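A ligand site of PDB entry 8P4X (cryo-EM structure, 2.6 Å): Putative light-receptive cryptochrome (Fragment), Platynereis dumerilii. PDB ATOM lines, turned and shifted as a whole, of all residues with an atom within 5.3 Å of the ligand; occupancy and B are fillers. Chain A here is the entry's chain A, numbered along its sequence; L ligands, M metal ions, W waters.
Merely in contact with the ligand: Val 423 (3.5 Å), Asn 427 (3.5 Å), Leu 287 (3.6 Å), Arg 324 (3.7 Å), Cys 424 (3.7 Å), Ser 284 (3.7 Å), Phe 327 (3.9 Å), Gly 419 (3.9 Å), Trp 323 (3.9 Å), Trp 428 (3.9 Å), Leu 321 (3.9 Å), Met 384 (3.95 Å) and Trp 383 (3.96 Å).
Hydrophobic or aromatic side chains within 4 Å of the ligand: Leu 287, Leu 321, Trp 323, Phe 327, His 386 and Val 423.
Of the 29 residues printed, 20 come within 4 Å of the ligand.
Along chain A the residues within 4 Å of the ligand span positions 254 to 428.
The nearest printed residue that does not touch the ligand is His 390 (4.05 Å).
The backbone carbonyl oxygen of Asp 418 sits close to the side-chain carboxylate of Asp 420.
OG of Ser 284 lies within hydrogen-bond range of OG of Ser 282.
NH2 of Arg 389 sits at hydrogen-bond distance from O of Met 384, at 2.8 Å.
The side-chain carboxylate (OD2) of Asp 420 is in salt-bridge range of the guanidinium group (NH1) of Arg 324.
The side-chain sulfur of Cys 424 sits close to the indole nitrogen of Trp 428 (3.8 Å).
A ring nitrogen (NE2) of His 386 is in hydrogen-bond range of the backbone carbonyl oxygen (O) of Phe 543, 3.3 Å away.
OD2 of Asp 418 is in hydrogen-bond range of OG of Ser 284 (3.2 Å).
The side-chain amide nitrogen (ND2) of Asn 427 sits at hydrogen-bond distance from the backbone carbonyl oxygen (O) of Val 423 (3.0 Å).
Water W3 bridges an oxygen (O7) of the ligand and the backbone carbonyl oxygen (O) of Ser 284.
Water W2 lies within hydrogen-bond range of the backbone carbonyl oxygen of Arg 281, an oxygen (O14) of the ligand and the backbone carbonyl oxygen of Pro 280.
Water W1 lies within hydrogen-bond range of N2 of the ligand (3.1 Å) and NE2 of Gln 320 (3.4 Å).
O8 of the ligand is in hydrogen-bond range of N of Asp 420, 3.5 Å away.
O of Asp 418 sits at hydrogen-bond distance from N7 of the ligand (3.1 Å).
NH2 of Arg 254 is in salt-bridge range of O2 of the ligand (2.9 Å).
A ring nitrogen (ND1) of His 386 sits at hydrogen-bond distance from an oxygen (O9) of the ligand (3.4 Å).
An oxygen (O13) of the ligand lies within hydrogen-bond range of the side-chain hydroxyl (OG) of Ser 282 (3.2 Å).
An oxygen (O11) of the ligand lies within hydrogen-bond range of the guanidinium group (NH2) of Arg 389 (2.9 Å).
OD1 of Asp 420 lies within hydrogen-bond range of N7 of the ligand, at 3.3 Å.
An oxygen (O1) of the ligand is in hydrogen-bond range of the side-chain amide nitrogen (NE2) of Gln 320, at 3.4 Å.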
ATOM      1  N   ARG A 254      31.126 -28.041  10.779  1.00  0.00           N
ATOM      2  CA  ARG A 254      30.590 -27.994   9.426  1.00  0.00           C
ATOM      3  C   ARG A 254      31.580 -27.324   8.472  1.00  0.00           C
ATOM      4  O   ARG A 254      31.829 -27.819   7.371  1.00  0.00           O
ATOM      5  CB  ARG A 254      29.251 -27.257   9.428  1.00  0.00           C
ATOM      6  CG  ARG A 254      28.636 -27.018   8.063  1.00  0.00           C
ATOM      7  CD  ARG A 254      28.121 -28.293   7.427  1.00  0.00           C
ATOM      8  NE  ARG A 254      26.774 -28.620   7.888  1.00  0.00           N
ATOM      9  CZ  ARG A 254      25.668 -28.078   7.401  1.00  0.00           C
ATOM     10  NH1 ARG A 254      25.714 -27.156   6.446  1.00  0.00           N
ATOM     11  NH2 ARG A 254      24.493 -28.461   7.877  1.00  0.00           N
ATOM     12  N   PRO A 280      23.242 -36.682  13.781  1.00  0.00           N
ATOM     13  CA  PRO A 280      22.616 -35.768  12.803  1.00  0.00           C
ATOM     14  C   PRO A 280      23.507 -34.607  12.409  1.00  0.00           C
ATOM     15  O   PRO A 280      23.701 -34.348  11.211  1.00  0.00           O
ATOM     16  CB  PRO A 280      21.368 -35.283  13.541  1.00  0.00           C
ATOM     17  CG  PRO A 280      21.096 -36.309  14.569  1.00  0.00           C
ATOM     18  CD  PRO A 280      22.433 -36.810  14.995  1.00  0.00           C
ATOM     19  N   ARG A 281      24.042 -33.875  13.394  1.00  0.00           N
ATOM     20  CA  ARG A 281      24.849 -32.686  13.139  1.00  0.00           C
ATOM     21  C   ARG A 281      24.025 -31.610  12.434  1.00  0.00           C
ATOM     22  O   ARG A 281      24.374 -31.124  11.357  1.00  0.00           O
ATOM     23  CB  ARG A 281      26.105 -33.029  12.328  1.00  0.00           C
ATOM     24  CG  ARG A 281      26.939 -34.154  12.898  1.00  0.00           C
ATOM     25  CD  ARG A 281      28.111 -34.483  11.997  1.00  0.00           C
ATOM     26  NE  ARG A 281      28.720 -35.764  12.309  1.00  0.00           N
ATOM     27  CZ  ARG A 281      29.673 -35.940  13.218  1.00  0.00           C
ATOM     28  NH1 ARG A 281      30.137 -34.932  13.938  1.00  0.00           N
ATOM     29  NH2 ARG A 281      30.170 -37.160  13.411  1.00  0.00           N
ATOM     30  N   SER A 282      22.911 -31.227  13.055  1.00  0.00           N
ATOM     31  CA  SER A 282      21.959 -30.283  12.497  1.00  0.00           C
ATOM     32  C   SER A 282      21.830 -29.069  13.405  1.00  0.00           C
ATOM     33  O   SER A 282      21.976 -29.179  14.621  1.00  0.00           O
ATOM     34  CB  SER A 282      20.586 -30.941  12.287  1.00  0.00           C
ATOM     35  OG  SER A 282      19.637 -30.010  11.819  1.00  0.00           O
ATOM     36  N   MET A 283      21.552 -27.917  12.796  1.00  0.00           N
ATOM     37  CA  MET A 283      21.391 -26.658  13.520  1.00  0.00           C
ATOM     38  C   MET A 283      20.033 -26.009  13.301  1.00  0.00           C
ATOM     39  O   MET A 283      19.854 -24.830  13.652  1.00  0.00           O
ATOM     40  CB  MET A 283      22.501 -25.691  13.118  1.00  0.00           C
ATOM     41  CG  MET A 283      23.850 -25.970  13.769  1.00  0.00           C
ATOM     42  SD  MET A 283      25.164 -24.908  13.151  1.00  0.00           S
ATOM     43  CE  MET A 283      25.404 -25.584  11.514  1.00  0.00           C
ATOM     44  N   SER A 284      19.063 -26.726  12.727  1.00  0.00           N
ATOM     45  CA  SER A 284      17.756 -26.130  12.494  1.00  0.00           C
ATOM     46  C   SER A 284      17.040 -25.753  13.785  1.00  0.00           C
ATOM     47  O   SER A 284      16.429 -24.677  13.836  1.00  0.00           O
ATOM     48  CB  SER A 284      16.904 -27.080  11.632  1.00  0.00           C
ATOM     49  OG  SER A 284      17.094 -28.432  11.972  1.00  0.00           O
ATOM     50  N   LEU A 287      18.488 -22.451  14.832  1.00  0.00           N
ATOM     51  CA  LEU A 287      18.017 -21.367  13.982  1.00  0.00           C
ATOM     52  C   LEU A 287      16.578 -20.978  14.316  1.00  0.00           C
ATOM     53  O   LEU A 287      16.231 -19.795  14.223  1.00  0.00           O
ATOM     54  CB  LEU A 287      18.127 -21.762  12.516  1.00  0.00           C
ATOM     55  CG  LEU A 287      19.537 -21.828  11.928  1.00  0.00           C
ATOM     56  CD1 LEU A 287      19.510 -22.496  10.567  1.00  0.00           C
ATOM     57  CD2 LEU A 287      20.129 -20.436  11.823  1.00  0.00           C
ATOM     58  N   GLN A 320      20.181 -23.785   0.368  1.00  0.00           N
ATOM     59  CA  GLN A 320      19.243 -24.315   1.345  1.00  0.00           C
ATOM     60  C   GLN A 320      18.706 -23.221   2.261  1.00  0.00           C
ATOM     61  O   GLN A 320      17.552 -23.297   2.709  1.00  0.00           O
ATOM     62  CB  GLN A 320      19.913 -25.410   2.170  1.00  0.00           C
ATOM     63  CG  GLN A 320      20.261 -26.662   1.376  1.00  0.00           C
ATOM     64  CD  GLN A 320      19.047 -27.428   0.915  1.00  0.00           C
ATOM     65  OE1 GLN A 320      18.294 -26.979   0.063  1.00  0.00           O
ATOM     66  NE2 GLN A 320      18.852 -28.606   1.489  1.00  0.00           N
ATOM     67  N   LEU A 321      19.517 -22.213   2.554  1.00  0.00           N
ATOM     68  CA  LEU A 321      19.081 -21.119   3.422  1.00  0.00           C
ATOM     69  C   LEU A 321      18.066 -20.201   2.751  1.00  0.00           C
ATOM     70  O   LEU A 321      17.496 -19.346   3.426  1.00  0.00           O
ATOM     71  CB  LEU A 321      20.292 -20.296   3.858  1.00  0.00           C
ATOM     72  CG  LEU A 321      21.384 -21.028   4.651  1.00  0.00           C
ATOM     73  CD1 LEU A 321      22.480 -20.060   5.033  1.00  0.00           C
ATOM     74  CD2 LEU A 321      20.816 -21.732   5.875  1.00  0.00           C
ATOM     75  N   TRP A 323      15.324 -21.425   0.877  1.00  0.00           N
ATOM     76  CA  TRP A 323      13.994 -22.014   1.033  1.00  0.00           C
ATOM     77  C   TRP A 323      13.319 -21.505   2.300  1.00  0.00           C
ATOM     78  O   TRP A 323      12.097 -21.263   2.312  1.00  0.00           O
ATOM     79  CB  TRP A 323      14.107 -23.544   1.076  1.00  0.00           C
ATOM     80  CG  TRP A 323      14.447 -24.188  -0.242  1.00  0.00           C
ATOM     81  CD1 TRP A 323      15.694 -24.431  -0.727  1.00  0.00           C
ATOM     82  CD2 TRP A 323      13.532 -24.690  -1.214  1.00  0.00           C
ATOM     83  NE1 TRP A 323      15.610 -25.047  -1.951  1.00  0.00           N
ATOM     84  CE2 TRP A 323      14.286 -25.212  -2.270  1.00  0.00           C
ATOM     85  CE3 TRP A 323      12.136 -24.739  -1.303  1.00  0.00           C
ATOM     86  CZ2 TRP A 323      13.714 -25.784  -3.399  1.00  0.00           C
ATOM     87  CZ3 TRP A 323      11.561 -25.291  -2.420  1.00  0.00           C
ATOM     88  CH2 TRP A 323      12.344 -25.817  -3.454  1.00  0.00           C
ATOM     89  N   ARG A 324      14.098 -21.355   3.373  1.00  0.00           N
ATOM     90  CA  ARG A 324      13.556 -20.828   4.617  1.00  0.00           C
ATOM     91  C   ARG A 324      12.952 -19.448   4.428  1.00  0.00           C
ATOM     92  O   ARG A 324      11.822 -19.181   4.852  1.00  0.00           O
ATOM     93  CB  ARG A 324      14.672 -20.806   5.663  1.00  0.00           C
ATOM     94  CG  ARG A 324      14.311 -20.284   7.033  1.00  0.00           C
ATOM     95  CD  ARG A 324      15.523 -20.367   7.944  1.00  0.00           C
ATOM     96  NE  ARG A 324      15.621 -19.240   8.858  1.00  0.00           N
ATOM     97  CZ  ARG A 324      15.259 -19.258  10.130  1.00  0.00           C
ATOM     98  NH1 ARG A 324      14.749 -20.343  10.695  1.00  0.00           N
ATOM     99  NH2 ARG A 324      15.407 -18.156  10.866  1.00  0.00           N
ATOM    100  N   PHE A 327       9.709 -19.559   2.250  1.00  0.00           N
ATOM    101  CA  PHE A 327       8.510 -19.935   2.999  1.00  0.00           C
ATOM    102  C   PHE A 327       8.119 -18.907   4.049  1.00  0.00           C
ATOM    103  O   PHE A 327       6.923 -18.767   4.352  1.00  0.00           O
ATOM    104  CB  PHE A 327       8.718 -21.305   3.655  1.00  0.00           C
ATOM    105  CG  PHE A 327       8.618 -22.461   2.700  1.00  0.00           C
ATOM    106  CD1 PHE A 327       7.537 -22.572   1.840  1.00  0.00           C
ATOM    107  CD2 PHE A 327       9.607 -23.420   2.655  1.00  0.00           C
ATOM    108  CE1 PHE A 327       7.449 -23.627   0.951  1.00  0.00           C
ATOM    109  CE2 PHE A 327       9.513 -24.475   1.774  1.00  0.00           C
ATOM    110  CZ  PHE A 327       8.437 -24.579   0.918  1.00  0.00           C
ATOM    111  N   TRP A 383      13.100 -35.335  16.195  1.00  0.00           N
ATOM    112  CA  TRP A 383      13.773 -34.907  14.983  1.00  0.00           C
ATOM    113  C   TRP A 383      13.766 -36.040  13.975  1.00  0.00           C
ATOM    114  O   TRP A 383      13.795 -37.221  14.341  1.00  0.00           O
ATOM    115  CB  TRP A 383      15.213 -34.455  15.270  1.00  0.00           C
ATOM    116  CG  TRP A 383      15.890 -33.827  14.099  1.00  0.00           C
ATOM    117  CD1 TRP A 383      15.843 -32.506  13.740  1.00  0.00           C
ATOM    118  CD2 TRP A 383      16.726 -34.470  13.137  1.00  0.00           C
ATOM    119  NE1 TRP A 383      16.590 -32.305  12.610  1.00  0.00           N
ATOM    120  CE2 TRP A 383      17.137 -33.488  12.212  1.00  0.00           C
ATOM    121  CE3 TRP A 383      17.161 -35.789  12.947  1.00  0.00           C
ATOM    122  CZ2 TRP A 383      17.970 -33.776  11.143  1.00  0.00           C
ATOM    123  CZ3 TRP A 383      17.982 -36.071  11.881  1.00  0.00           C
ATOM    124  CH2 TRP A 383      18.378 -35.069  10.985  1.00  0.00           C
ATOM    125  N   MET A 384      13.729 -35.688  12.695  1.00  0.00           N
ATOM    126  CA  MET A 384      13.688 -36.668  11.619  1.00  0.00           C
ATOM    127  C   MET A 384      14.379 -36.097  10.392  1.00  0.00           C
ATOM    128  O   MET A 384      14.461 -34.884  10.214  1.00  0.00           O
ATOM    129  CB  MET A 384      12.244 -37.049  11.284  1.00  0.00           C
ATOM    130  CG  MET A 384      12.098 -38.399  10.610  1.00  0.00           C
ATOM    131  SD  MET A 384      10.650 -38.472   9.546  1.00  0.00           S
ATOM    132  CE  MET A 384       9.361 -37.882  10.638  1.00  0.00           C
ATOM    133  N   HIS A 385      14.867 -36.995   9.539  1.00  0.00           N
ATOM    134  CA  HIS A 385      15.487 -36.600   8.284  1.00  0.00           C
ATOM    135  C   HIS A 385      14.431 -36.185   7.261  1.00  0.00           C
ATOM    136  O   HIS A 385      13.268 -36.582   7.329  1.00  0.00           O
ATOM    137  CB  HIS A 385      16.339 -37.750   7.731  1.00  0.00           C
ATOM    138  CG  HIS A 385      17.291 -37.333   6.658  1.00  0.00           C
ATOM    139  ND1 HIS A 385      16.894 -37.103   5.359  1.00  0.00           N
ATOM    140  CD2 HIS A 385      18.629 -37.118   6.687  1.00  0.00           C
ATOM    141  CE1 HIS A 385      17.944 -36.761   4.633  1.00  0.00           C
ATOM    142  NE2 HIS A 385      19.009 -36.765   5.411  1.00  0.00           N
ATOM    143  N   HIS A 386      14.868 -35.364   6.309  1.00  0.00           N
ATOM    144  CA  HIS A 386      13.962 -34.814   5.295  1.00  0.00           C
ATOM    145  C   HIS A 386      13.205 -35.905   4.547  1.00  0.00           C
ATOM    146  O   HIS A 386      11.999 -35.790   4.298  1.00  0.00           O
ATOM    147  CB  HIS A 386      14.780 -33.954   4.322  1.00  0.00           C
ATOM    148  CG  HIS A 386      13.948 -33.249   3.299  1.00  0.00           C
ATOM    149  ND1 HIS A 386      13.169 -32.144   3.589  1.00  0.00           N
ATOM    150  CD2 HIS A 386      13.778 -33.483   1.969  1.00  0.00           C
ATOM    151  CE1 HIS A 386      12.552 -31.741   2.498  1.00  0.00           C
ATOM    152  NE2 HIS A 386      12.909 -32.524   1.500  1.00  0.00           N
ATOM    153  N   ARG A 389      10.256 -37.264   6.518  1.00  0.00           N
ATOM    154  CA  ARG A 389       9.135 -36.331   6.574  1.00  0.00           C
ATOM    155  C   ARG A 389       8.364 -36.325   5.264  1.00  0.00           C
ATOM    156  O   ARG A 389       7.127 -36.367   5.259  1.00  0.00           O
ATOM    157  CB  ARG A 389       9.645 -34.923   6.887  1.00  0.00           C
ATOM    158  CG  ARG A 389      10.534 -34.834   8.103  1.00  0.00           C
ATOM    159  CD  ARG A 389      10.933 -33.407   8.395  1.00  0.00           C
ATOM    160  NE  ARG A 389      12.110 -33.330   9.252  1.00  0.00           N
ATOM    161  CZ  ARG A 389      12.460 -32.268   9.963  1.00  0.00           C
ATOM    162  NH1 ARG A 389      11.709 -31.182   9.997  1.00  0.00           N
ATOM    163  NH2 ARG A 389      13.577 -32.310  10.678  1.00  0.00           N
ATOM    164  N   HIS A 390       9.078 -36.276   4.136  1.00  0.00           N
ATOM    165  CA  HIS A 390       8.405 -36.340   2.834  1.00  0.00           C
ATOM    166  C   HIS A 390       7.611 -37.629   2.690  1.00  0.00           C
ATOM    167  O   HIS A 390       6.457 -37.617   2.234  1.00  0.00           O
ATOM    168  CB  HIS A 390       9.430 -36.207   1.711  1.00  0.00           C
ATOM    169  CG  HIS A 390       8.845 -36.320   0.348  1.00  0.00           C
ATOM    170  ND1 HIS A 390       8.013 -35.358  -0.194  1.00  0.00           N
ATOM    171  CD2 HIS A 390       8.960 -37.280  -0.595  1.00  0.00           C
ATOM    172  CE1 HIS A 390       7.647 -35.729  -1.405  1.00  0.00           C
ATOM    173  NE2 HIS A 390       8.210 -36.888  -1.675  1.00  0.00           N
ATOM    174  N   ALA A 393       4.432 -37.544   4.976  1.00  0.00           N
ATOM    175  CA  ALA A 393       3.454 -36.587   4.474  1.00  0.00           C
ATOM    176  C   ALA A 393       2.750 -37.129   3.233  1.00  0.00           C
ATOM    177  O   ALA A 393       1.518 -37.051   3.126  1.00  0.00           O
ATOM    178  CB  ALA A 393       4.129 -35.260   4.177  1.00  0.00           C
ATOM    179  N   PHE A 412       3.244 -32.480  14.026  1.00  0.00           N
ATOM    180  CA  PHE A 412       4.548 -31.851  13.853  1.00  0.00           C
ATOM    181  C   PHE A 412       4.685 -30.607  14.727  1.00  0.00           C
ATOM    182  O   PHE A 412       5.743 -30.393  15.337  1.00  0.00           O
ATOM    183  CB  PHE A 412       4.752 -31.507  12.377  1.00  0.00           C
ATOM    184  CG  PHE A 412       5.222 -32.670  11.544  1.00  0.00           C
ATOM    185  CD1 PHE A 412       4.604 -33.893  11.639  1.00  0.00           C
ATOM    186  CD2 PHE A 412       6.271 -32.513  10.654  1.00  0.00           C
ATOM    187  CE1 PHE A 412       5.028 -34.960  10.877  1.00  0.00           C
ATOM    188  CE2 PHE A 412       6.701 -33.579   9.884  1.00  0.00           C
ATOM    189  CZ  PHE A 412       6.082 -34.803  10.004  1.00  0.00           C
ATOM    190  N   ASP A 418      11.906 -28.087  15.787  1.00  0.00           N
ATOM    191  CA  ASP A 418      11.979 -26.914  14.918  1.00  0.00           C
ATOM    192  C   ASP A 418      10.665 -26.725  14.175  1.00  0.00           C
ATOM    193  O   ASP A 418      10.634 -26.541  12.952  1.00  0.00           O
ATOM    194  CB  ASP A 418      13.149 -27.038  13.940  1.00  0.00           C
ATOM    195  CG  ASP A 418      13.053 -28.285  13.071  1.00  0.00           C
ATOM    196  OD1 ASP A 418      12.074 -29.042  13.233  1.00  0.00           O
ATOM    197  OD2 ASP A 418      13.945 -28.489  12.229  1.00  0.00           O
ATOM    198  N   GLY A 419       9.560 -26.767  14.902  1.00  0.00           N
ATOM    199  CA  GLY A 419       8.251 -26.634  14.298  1.00  0.00           C
ATOM    200  C   GLY A 419       7.866 -25.199  14.015  1.00  0.00           C
ATOM    201  O   GLY A 419       6.915 -24.674  14.618  1.00  0.00           O
ATOM    202  N   ASP A 420       8.578 -24.553  13.099  1.00  0.00           N
ATOM    203  CA  ASP A 420       8.260 -23.184  12.738  1.00  0.00           C
ATOM    204  C   ASP A 420       6.836 -23.096  12.206  1.00  0.00           C
ATOM    205  O   ASP A 420       6.366 -23.970  11.465  1.00  0.00           O
ATOM    206  CB  ASP A 420       9.244 -22.664  11.682  1.00  0.00           C
ATOM    207  CG  ASP A 420      10.680 -22.837  12.091  1.00  0.00           C
ATOM    208  OD1 ASP A 420      11.107 -23.991  12.322  1.00  0.00           O
ATOM    209  OD2 ASP A 420      11.402 -21.823  12.176  1.00  0.00           O
ATOM    210  N   VAL A 423       7.137 -22.393   8.091  1.00  0.00           N
ATOM    211  CA  VAL A 423       7.933 -23.287   7.246  1.00  0.00           C
ATOM    212  C   VAL A 423       7.266 -24.658   7.143  1.00  0.00           C
ATOM    213  O   VAL A 423       7.193 -25.251   6.054  1.00  0.00           O
ATOM    214  CB  VAL A 423       9.370 -23.388   7.786  1.00  0.00           C
ATOM    215  CG1 VAL A 423      10.225 -24.291   6.910  1.00  0.00           C
ATOM    216  CG2 VAL A 423      10.002 -22.020   7.887  1.00  0.00           C
ATOM    217  N   CYS A 424       6.798 -25.197   8.264  1.00  0.00           N
ATOM    218  CA  CYS A 424       6.181 -26.520   8.253  1.00  0.00           C
ATOM    219  C   CYS A 424       4.906 -26.541   7.414  1.00  0.00           C
ATOM    220  O   CYS A 424       4.710 -27.449   6.602  1.00  0.00           O
ATOM    221  CB  CYS A 424       5.906 -26.956   9.693  1.00  0.00           C
ATOM    222  SG  CYS A 424       5.562 -28.716   9.902  1.00  0.00           S
ATOM    223  N   ASN A 427       5.839 -26.357   3.712  1.00  0.00           N
ATOM    224  CA  ASN A 427       6.296 -27.648   3.189  1.00  0.00           C
ATOM    225  C   ASN A 427       5.129 -28.622   3.016  1.00  0.00           C
ATOM    226  O   ASN A 427       5.094 -29.382   2.035  1.00  0.00           O
ATOM    227  CB  ASN A 427       7.355 -28.248   4.115  1.00  0.00           C
ATOM    228  CG  ASN A 427       8.750 -27.789   3.762  1.00  0.00           C
ATOM    229  OD1 ASN A 427       9.383 -28.314   2.852  1.00  0.00           O
ATOM    230  ND2 ASN A 427       9.252 -26.813   4.496  1.00  0.00           N
ATOM    231  N   TRP A 428       4.188 -28.642   3.959  1.00  0.00           N
ATOM    232  CA  TRP A 428       3.028 -29.516   3.811  1.00  0.00           C
ATOM    233  C   TRP A 428       2.217 -29.151   2.569  1.00  0.00           C
ATOM    234  O   TRP A 428       1.844 -30.038   1.787  1.00  0.00           O
ATOM    235  CB  TRP A 428       2.142 -29.437   5.054  1.00  0.00           C
ATOM    236  CG  TRP A 428       2.557 -30.383   6.147  1.00  0.00           C
ATOM    237  CD1 TRP A 428       3.385 -30.115   7.189  1.00  0.00           C
ATOM    238  CD2 TRP A 428       2.134 -31.745   6.307  1.00  0.00           C
ATOM    239  NE1 TRP A 428       3.524 -31.228   7.984  1.00  0.00           N
ATOM    240  CE2 TRP A 428       2.757 -32.240   7.460  1.00  0.00           C
ATOM    241  CE3 TRP A 428       1.285 -32.588   5.579  1.00  0.00           C
ATOM    242  CZ2 TRP A 428       2.567 -33.546   7.904  1.00  0.00           C
ATOM    243  CZ3 TRP A 428       1.100 -33.887   6.027  1.00  0.00           C
ATOM    244  CH2 TRP A 428       1.738 -34.352   7.181  1.00  0.00           C
ATOM    245  N   VAL A 431       4.215 -30.257  -0.610  1.00  0.00           N
ATOM    246  CA  VAL A 431       4.187 -31.687  -0.908  1.00  0.00           C
ATOM    247  C   VAL A 431       2.793 -32.115  -1.360  1.00  0.00           C
ATOM    248  O   VAL A 431       2.639 -32.821  -2.366  1.00  0.00           O
ATOM    249  CB  VAL A 431       4.655 -32.500   0.309  1.00  0.00           C
ATOM    250  CG1 VAL A 431       4.390 -33.979   0.116  1.00  0.00           C
ATOM    251  CG2 VAL A 431       6.132 -32.252   0.560  1.00  0.00           C
ATOM    252  N   PHE A 543      14.495 -32.295  -4.700  1.00  0.00           N
ATOM    253  CA  PHE A 543      13.867 -32.145  -3.394  1.00  0.00           C
ATOM    254  C   PHE A 543      13.717 -33.489  -2.696  1.00  0.00           C
ATOM    255  O   PHE A 543      13.825 -33.566  -1.470  1.00  0.00           O
ATOM    256  CB  PHE A 543      12.495 -31.476  -3.585  1.00  0.00           C
ATOM    257  CG  PHE A 543      11.798 -31.118  -2.306  1.00  0.00           C
ATOM    258  CD1 PHE A 543      11.003 -32.028  -1.646  1.00  0.00           C
ATOM    259  CD2 PHE A 543      11.904 -29.836  -1.792  1.00  0.00           C
ATOM    260  CE1 PHE A 543      10.348 -31.695  -0.488  1.00  0.00           C
ATOM    261  CE2 PHE A 543      11.248 -29.490  -0.634  1.00  0.00           C
ATOM    262  CZ  PHE A 543      10.467 -30.420   0.022  1.00  0.00           C
HETATM  263  P1  LIG L   1      20.807 -28.894   5.846  1.00  0.00           P
HETATM  264  O1  LIG L   1      20.576 -28.764   4.390  1.00  0.00           O
HETATM  265  O2  LIG L   1      22.223 -29.345   6.234  1.00  0.00           O
HETATM  266  O3  LIG L   1      20.465 -27.557   6.599  1.00  0.00           O
HETATM  267  C1  LIG L   1      20.498 -26.280   5.920  1.00  0.00           C
HETATM  268  C2  LIG L   1      19.435 -25.382   6.485  1.00  0.00           C
HETATM  269  O4  LIG L   1      18.581 -24.928   5.417  1.00  0.00           O
HETATM  270  C3  LIG L   1      18.489 -26.041   7.486  1.00  0.00           C
HETATM  271  O5  LIG L   1      19.024 -25.996   8.794  1.00  0.00           O
HETATM  272  C4  LIG L   1      17.231 -25.177   7.357  1.00  0.00           C
HETATM  273  O6  LIG L   1      17.289 -24.011   8.179  1.00  0.00           O
HETATM  274  C5  LIG L   1      17.246 -24.799   5.878  1.00  0.00           C
HETATM  275  N1  LIG L   1      16.396 -25.636   5.023  1.00  0.00           N
HETATM  276  C6  LIG L   1      16.774 -26.728   4.312  1.00  0.00           C
HETATM  277  N2  LIG L   1      15.799 -27.283   3.620  1.00  0.00           N
HETATM  278  C7  LIG L   1      14.704 -26.489   3.914  1.00  0.00           C
HETATM  279  C8  LIG L   1      13.362 -26.542   3.513  1.00  0.00           C
HETATM  280  N3  LIG L   1      12.866 -27.469   2.685  1.00  0.00           N
HETATM  281  N4  LIG L   1      12.519 -25.590   3.984  1.00  0.00           N
HETATM  282  C9  LIG L   1      12.998 -24.665   4.812  1.00  0.00           C
HETATM  283  N5  LIG L   1      14.248 -24.513   5.262  1.00  0.00           N
HETATM  284  C10 LIG L   1      15.057 -25.461   4.777  1.00  0.00           C
HETATM  285  N6  LIG L   1      12.678 -27.353   8.148  1.00  0.00           N
HETATM  286  C11 LIG L   1      12.700 -26.495   9.202  1.00  0.00           C
HETATM  287  O7  LIG L   1      13.699 -25.819   9.466  1.00  0.00           O
HETATM  288  N7  LIG L   1      11.584 -26.360  10.007  1.00  0.00           N
HETATM  289  C12 LIG L   1      10.396 -27.038   9.850  1.00  0.00           C
HETATM  290  O8  LIG L   1       9.471 -26.830  10.629  1.00  0.00           O
HETATM  291  C13 LIG L   1      10.379 -27.938   8.722  1.00  0.00           C
HETATM  292  N8  LIG L   1       9.281 -28.616   8.507  1.00  0.00           N
HETATM  293  C14 LIG L   1       9.265 -29.481   7.433  1.00  0.00           C
HETATM  294  C15 LIG L   1       8.097 -30.214   7.187  1.00  0.00           C
HETATM  295  C16 LIG L   1       8.031 -31.105   6.123  1.00  0.00           C
HETATM  296  C17 LIG L   1       6.749 -31.876   5.888  1.00  0.00           C
HETATM  297  C18 LIG L   1       9.129 -31.270   5.276  1.00  0.00           C
HETATM  298  C19 LIG L   1       9.090 -32.229   4.116  1.00  0.00           C
HETATM  299  C20 LIG L   1      10.292 -30.544   5.519  1.00  0.00           C
HETATM  300  C21 LIG L   1      10.369 -29.652   6.591  1.00  0.00           C
HETATM  301  N9  LIG L   1      11.535 -28.905   6.862  1.00  0.00           N
HETATM  302  C22 LIG L   1      11.568 -28.032   7.924  1.00  0.00           C
HETATM  303  C23 LIG L   1      12.729 -29.034   6.003  1.00  0.00           C
HETATM  304  C24 LIG L   1      13.657 -30.166   6.405  1.00  0.00           C
HETATM  305  O9  LIG L   1      12.909 -31.278   6.900  1.00  0.00           O
HETATM  306  C25 LIG L   1      14.621 -29.680   7.490  1.00  0.00           C
HETATM  307  O10 LIG L   1      15.116 -28.390   7.140  1.00  0.00           O
HETATM  308  C26 LIG L   1      15.829 -30.605   7.690  1.00  0.00           C
HETATM  309  O11 LIG L   1      15.649 -31.360   8.881  1.00  0.00           O
HETATM  310  C27 LIG L   1      17.129 -29.833   7.762  1.00  0.00           C
HETATM  311  O12 LIG L   1      18.180 -30.720   8.173  1.00  0.00           O
HETATM  312  P2  LIG L   1      19.696 -30.321   7.997  1.00  0.00           P
HETATM  313  O13 LIG L   1      19.995 -29.070   8.833  1.00  0.00           O
HETATM  314  O14 LIG L   1      20.578 -31.471   8.275  1.00  0.00           O
HETATM  315  O15 LIG L   1      19.781 -29.923   6.472  1.00  0.00           O
HETATM  316 MG    MG M   1      22.215 -27.612   9.779  1.00  0.00          MG
HETATM  317  O   HOH W   1      16.209 -30.232   2.921  1.00  0.00           O
HETATM  318  O   HOH W   2      23.457 -31.746   8.939  1.00  0.00           O
HETATM  319  O   HOH W   3      15.114 -23.859  11.025  1.00  0.00           O
HETATM  320  O   HOH W   4      17.984 -33.497   6.731  1.00  0.00           O
